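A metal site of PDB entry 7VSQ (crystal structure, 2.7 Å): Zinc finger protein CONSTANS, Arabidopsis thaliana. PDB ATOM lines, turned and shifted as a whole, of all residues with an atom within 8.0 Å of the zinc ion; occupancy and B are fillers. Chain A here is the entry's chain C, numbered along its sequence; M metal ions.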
ATOM      1  N   TYR A  23       0.555  15.471  16.601  1.00  0.00           N
ATOM      2  CA  TYR A  23       1.134  15.528  17.939  1.00  0.00           C
ATOM      3  C   TYR A  23       2.347  14.603  18.024  1.00  0.00           C
ATOM      4  O   TYR A  23       2.259  13.418  17.708  1.00  0.00           O
ATOM      5  CB  TYR A  23       0.122  15.132  19.014  1.00  0.00           C
ATOM      6  CG  TYR A  23       0.735  15.079  20.402  1.00  0.00           C
ATOM      7  CD1 TYR A  23       1.324  16.210  20.966  1.00  0.00           C
ATOM      8  CD2 TYR A  23       0.750  13.912  21.142  1.00  0.00           C
ATOM      9  CE1 TYR A  23       1.888  16.177  22.221  1.00  0.00           C
ATOM     10  CE2 TYR A  23       1.317  13.868  22.411  1.00  0.00           C
ATOM     11  CZ  TYR A  23       1.883  15.001  22.937  1.00  0.00           C
ATOM     12  OH  TYR A  23       2.456  14.977  24.197  1.00  0.00           O
ATOM     13  N   CYS A  24       3.475  15.148  18.477  1.00  0.00           N
ATOM     14  CA  CYS A  24       4.617  14.324  18.814  1.00  0.00           C
ATOM     15  C   CYS A  24       4.811  14.246  20.321  1.00  0.00           C
ATOM     16  O   CYS A  24       5.005  15.270  20.975  1.00  0.00           O
ATOM     17  CB  CYS A  24       5.894  14.851  18.174  1.00  0.00           C
ATOM     18  SG  CYS A  24       7.304  13.817  18.565  1.00  0.00           S
ATOM     19  N   HIS A  25       4.764  13.039  20.865  1.00  0.00           N
ATOM     20  CA  HIS A  25       5.005  12.854  22.279  1.00  0.00           C
ATOM     21  C   HIS A  25       6.507  12.984  22.561  1.00  0.00           C
ATOM     22  O   HIS A  25       6.909  13.480  23.616  1.00  0.00           O
ATOM     23  CB  HIS A  25       4.489  11.501  22.758  1.00  0.00           C
ATOM     24  CG  HIS A  25       4.767  11.234  24.199  1.00  0.00           C
ATOM     25  ND1 HIS A  25       4.225  11.994  25.210  1.00  0.00           N
ATOM     26  CD2 HIS A  25       5.551  10.305  24.800  1.00  0.00           C
ATOM     27  CE1 HIS A  25       4.650  11.538  26.380  1.00  0.00           C
ATOM     28  NE2 HIS A  25       5.458  10.516  26.155  1.00  0.00           N
ATOM     29  N   ALA A  26       7.312  12.497  21.626  1.00  0.00           N
ATOM     30  CA  ALA A  26       8.767  12.586  21.745  1.00  0.00           C
ATOM     31  C   ALA A  26       9.226  14.047  21.815  1.00  0.00           C
ATOM     32  O   ALA A  26      10.044  14.405  22.658  1.00  0.00           O
ATOM     33  CB  ALA A  26       9.433  11.854  20.584  1.00  0.00           C
ATOM     34  N   ASP A  27       8.703  14.879  20.934  1.00  0.00           N
ATOM     35  CA  ASP A  27       8.943  16.317  21.018  1.00  0.00           C
ATOM     36  C   ASP A  27       8.040  16.936  22.096  1.00  0.00           C
ATOM     37  O   ASP A  27       8.234  18.085  22.486  1.00  0.00           O
ATOM     38  CB  ASP A  27       8.733  17.013  19.667  1.00  0.00           C
ATOM     39  CG  ASP A  27       9.827  16.682  18.668  1.00  0.00           C
ATOM     40  OD1 ASP A  27       9.679  15.702  17.922  1.00  0.00           O
ATOM     41  OD2 ASP A  27      10.859  17.393  18.649  1.00  0.00           O
ATOM     42  N   SER A  28       7.062  16.151  22.534  1.00  0.00           N
ATOM     43  CA  SER A  28       6.087  16.533  23.551  1.00  0.00           C
ATOM     44  C   SER A  28       5.371  17.856  23.253  1.00  0.00           C
ATOM     45  O   SER A  28       5.151  18.668  24.156  1.00  0.00           O
ATOM     46  CB  SER A  28       6.765  16.624  24.922  1.00  0.00           C
ATOM     47  OG  SER A  28       5.870  17.140  25.896  1.00  0.00           O
ATOM     48  N   ALA A  29       4.989  18.036  22.000  1.00  0.00           N
ATOM     49  CA  ALA A  29       4.296  19.243  21.572  1.00  0.00           C
ATOM     50  C   ALA A  29       3.279  18.965  20.481  1.00  0.00           C
ATOM     51  O   ALA A  29       3.391  17.985  19.746  1.00  0.00           O
ATOM     52  CB  ALA A  29       5.283  20.298  21.109  1.00  0.00           C
ATOM     53  N   LEU A  31       1.763  20.030  16.958  1.00  0.00           N
ATOM     54  CA  LEU A  31       2.310  20.691  15.794  1.00  0.00           C
ATOM     55  C   LEU A  31       1.251  20.808  14.721  1.00  0.00           C
ATOM     56  O   LEU A  31       0.229  20.096  14.745  1.00  0.00           O
ATOM     57  CB  LEU A  31       3.529  19.930  15.233  1.00  0.00           C
ATOM     58  CG  LEU A  31       4.905  19.909  15.892  1.00  0.00           C
ATOM     59  CD1 LEU A  31       4.856  19.335  17.305  1.00  0.00           C
ATOM     60  CD2 LEU A  31       5.843  19.072  15.047  1.00  0.00           C
ATOM     61  N   ASP A  36       6.083  20.122  11.176  1.00  0.00           N
ATOM     62  CA  ASP A  36       6.482  18.752  11.434  1.00  0.00           C
ATOM     63  C   ASP A  36       7.527  18.235  10.443  1.00  0.00           C
ATOM     64  O   ASP A  36       8.555  17.683  10.845  1.00  0.00           O
ATOM     65  CB  ASP A  36       5.272  17.843  11.422  1.00  0.00           C
ATOM     66  CG  ASP A  36       5.652  16.457  11.751  1.00  0.00           C
ATOM     67  OD1 ASP A  36       5.747  15.624  10.822  1.00  0.00           O
ATOM     68  OD2 ASP A  36       5.947  16.263  12.953  1.00  0.00           O
ATOM     69  N   VAL A  39      10.777  20.397  11.190  1.00  0.00           N
ATOM     70  CA  VAL A  39      11.389  20.160  12.499  1.00  0.00           C
ATOM     71  C   VAL A  39      12.144  18.846  12.472  1.00  0.00           C
ATOM     72  O   VAL A  39      13.238  18.734  13.010  1.00  0.00           O
ATOM     73  CB  VAL A  39      10.324  20.101  13.623  1.00  0.00           C
ATOM     74  CG1 VAL A  39      10.929  19.594  14.935  1.00  0.00           C
ATOM     75  CG2 VAL A  39       9.646  21.453  13.819  1.00  0.00           C
ATOM     76  N   HIS A  40      11.536  17.865  11.818  1.00  0.00           N
ATOM     77  CA  HIS A  40      12.076  16.517  11.797  1.00  0.00           C
ATOM     78  C   HIS A  40      12.886  16.232  10.538  1.00  0.00           C
ATOM     79  O   HIS A  40      13.273  15.092  10.286  1.00  0.00           O
ATOM     80  CB  HIS A  40      10.949  15.496  11.968  1.00  0.00           C
ATOM     81  CG  HIS A  40      10.250  15.583  13.294  1.00  0.00           C
ATOM     82  ND1 HIS A  40       9.529  16.693  13.678  1.00  0.00           N
ATOM     83  CD2 HIS A  40      10.231  14.748  14.348  1.00  0.00           C
ATOM     84  CE1 HIS A  40       9.049  16.499  14.896  1.00  0.00           C
ATOM     85  NE2 HIS A  40       9.466  15.323  15.324  1.00  0.00           N
ATOM     86  N   VAL A  45      17.956  11.569  14.136  1.00  0.00           N
ATOM     87  CA  VAL A  45      17.286  11.352  15.419  1.00  0.00           C
ATOM     88  C   VAL A  45      15.885  11.923  15.378  1.00  0.00           C
ATOM     89  O   VAL A  45      14.969  11.377  15.974  1.00  0.00           O
ATOM     90  CB  VAL A  45      18.083  11.981  16.566  1.00  0.00           C
ATOM     91  CG1 VAL A  45      17.609  11.439  17.916  1.00  0.00           C
ATOM     92  CG2 VAL A  45      19.564  11.729  16.365  1.00  0.00           C
ATOM     93  N   ALA A  46      15.737  13.041  14.682  1.00  0.00           N
ATOM     94  CA  ALA A  46      14.427  13.608  14.404  1.00  0.00           C
ATOM     95  C   ALA A  46      13.646  12.674  13.496  1.00  0.00           C
ATOM     96  O   ALA A  46      12.417  12.591  13.566  1.00  0.00           O
ATOM     97  CB  ALA A  46      14.568  14.976  13.777  1.00  0.00           C
ATOM     98  N   SER A  47      14.373  11.954  12.648  1.00  0.00           N
ATOM     99  CA  SER A  47      13.799  11.002  11.699  1.00  0.00           C
ATOM    100  C   SER A  47      12.989   9.887  12.350  1.00  0.00           C
ATOM    101  O   SER A  47      11.979   9.451  11.807  1.00  0.00           O
ATOM    102  CB  SER A  47      14.902  10.373  10.853  1.00  0.00           C
ATOM    103  OG  SER A  47      14.486   9.128  10.317  1.00  0.00           O
ATOM    104  N   ARG A  48      13.421   9.421  13.524  1.00  0.00           N
ATOM    105  CA  ARG A  48      12.738   8.306  14.156  1.00  0.00           C
ATOM    106  C   ARG A  48      11.951   8.889  15.349  1.00  0.00           C
ATOM    107  O   ARG A  48      11.662   8.233  16.328  1.00  0.00           O
ATOM    108  CB  ARG A  48      13.753   7.202  14.520  1.00  0.00           C
ATOM    109  CG  ARG A  48      13.392   5.978  15.403  1.00  0.00           C
ATOM    110  CD  ARG A  48      11.918   5.583  15.481  1.00  0.00           C
ATOM    111  NE  ARG A  48      11.342   4.829  14.378  1.00  0.00           N
ATOM    112  CZ  ARG A  48      10.123   5.063  13.910  1.00  0.00           C
ATOM    113  NH1 ARG A  48       9.637   4.334  12.915  1.00  0.00           N
ATOM    114  NH2 ARG A  48       9.396   6.046  14.428  1.00  0.00           N
ATOM    115  N   HIS A  49      11.633  10.176  15.260  1.00  0.00           N
ATOM    116  CA  HIS A  49      10.531  10.673  16.070  1.00  0.00           C
ATOM    117  C   HIS A  49       9.249  10.107  15.482  1.00  0.00           C
ATOM    118  O   HIS A  49       9.172   9.852  14.275  1.00  0.00           O
ATOM    119  CB  HIS A  49      10.495  12.193  16.139  1.00  0.00           C
ATOM    120  CG  HIS A  49      11.358  12.754  17.225  1.00  0.00           C
ATOM    121  ND1 HIS A  49      10.844  13.532  18.250  1.00  0.00           N
ATOM    122  CD2 HIS A  49      12.676  12.627  17.476  1.00  0.00           C
ATOM    123  CE1 HIS A  49      11.824  13.867  19.072  1.00  0.00           C
ATOM    124  NE2 HIS A  49      12.945  13.336  18.624  1.00  0.00           N
ATOM    125  N   LYS A  50       8.245   9.915  16.327  1.00  0.00           N
ATOM    126  CA  LYS A  50       6.962   9.393  15.886  1.00  0.00           C
ATOM    127  C   LYS A  50       5.898  10.454  16.076  1.00  0.00           C
ATOM    128  O   LYS A  50       5.810  11.069  17.128  1.00  0.00           O
ATOM    129  CB  LYS A  50       6.545   8.141  16.682  1.00  0.00           C
ATOM    130  CG  LYS A  50       7.577   7.022  16.917  1.00  0.00           C
ATOM    131  CD  LYS A  50       8.764   7.452  17.772  1.00  0.00           C
ATOM    132  CE  LYS A  50       9.698   6.313  18.092  1.00  0.00           C
ATOM    133  NZ  LYS A  50      10.772   6.744  19.042  1.00  0.00           N
ATOM    134  N   ARG A  51       5.086  10.663  15.047  1.00  0.00           N
ATOM    135  CA  ARG A  51       4.133  11.752  15.090  1.00  0.00           C
ATOM    136  C   ARG A  51       2.735  11.233  14.826  1.00  0.00           C
ATOM    137  O   ARG A  51       2.488  10.525  13.841  1.00  0.00           O
ATOM    138  CB  ARG A  51       4.522  12.831  14.105  1.00  0.00           C
ATOM    139  CG  ARG A  51       5.471  12.359  13.043  1.00  0.00           C
ATOM    140  CD  ARG A  51       6.370  13.496  12.779  1.00  0.00           C
ATOM    141  NE  ARG A  51       7.277  13.357  11.647  1.00  0.00           N
ATOM    142  CZ  ARG A  51       8.502  12.873  11.741  1.00  0.00           C
ATOM    143  NH1 ARG A  51       8.960  12.454  12.916  1.00  0.00           N
ATOM    144  NH2 ARG A  51       9.276  12.806  10.666  1.00  0.00           N
ATOM    145  N   VAL A  52       1.814  11.617  15.690  1.00  0.00           N
ATOM    146  CA  VAL A  52       0.459  11.109  15.612  1.00  0.00           C
ATOM    147  C   VAL A  52      -0.505  12.262  15.343  1.00  0.00           C
ATOM    148  O   VAL A  52      -0.160  13.424  15.555  1.00  0.00           O
ATOM    149  CB  VAL A  52       0.123  10.335  16.918  1.00  0.00           C
ATOM    150  CG1 VAL A  52      -1.170  10.804  17.595  1.00  0.00           C
ATOM    151  CG2 VAL A  52       0.123   8.833  16.653  1.00  0.00           C
HETATM  152 ZN    ZN M   1       8.624  14.548  17.020  1.00  0.00          ZN
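OD1 of Asp 27 binds the zinc ion (1.8 Å).
A ring nitrogen (NE2) of His 40 binds the zinc ion (2.0 Å).
The side-chain sulfur (SG) of Cys 24 is bound to the zinc ion (2.2 Å).
Slightly farther from the zinc ion lies a ring nitrogen (ND1) of His 49 (2.7 Å).
The nearest printed residue that does not touch the zinc ion is Lys 50 (4.5 Å).
The side-chain carboxylate of Asp 27 lies close to a ring nitrogen (ND1) of His 49.
ND1 of His 40 lies within hydrogen-bond range of O of Asp 36, at 3.2 Å.
The side-chain sulfur of Cys 24 sits close to a ring nitrogen (ND1) of His 49 (3.6 Å).
The side-chain sulfur (SG) of Cys 24 lies close to the backbone carbonyl oxygen (O) of Lys 50 (3.4 Å).
The side-chain sulfur of Cys 24 lies close to the backbone NH of Ala 26 (3.3 Å).
O of Cys 24 sits at hydrogen-bond distance from N of Ala 29.
The backbone carbonyl oxygen (O) of His 49 lies within hydrogen-bond range of the guanidinium group (NH1) of Arg 51, 2.9 Å away.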
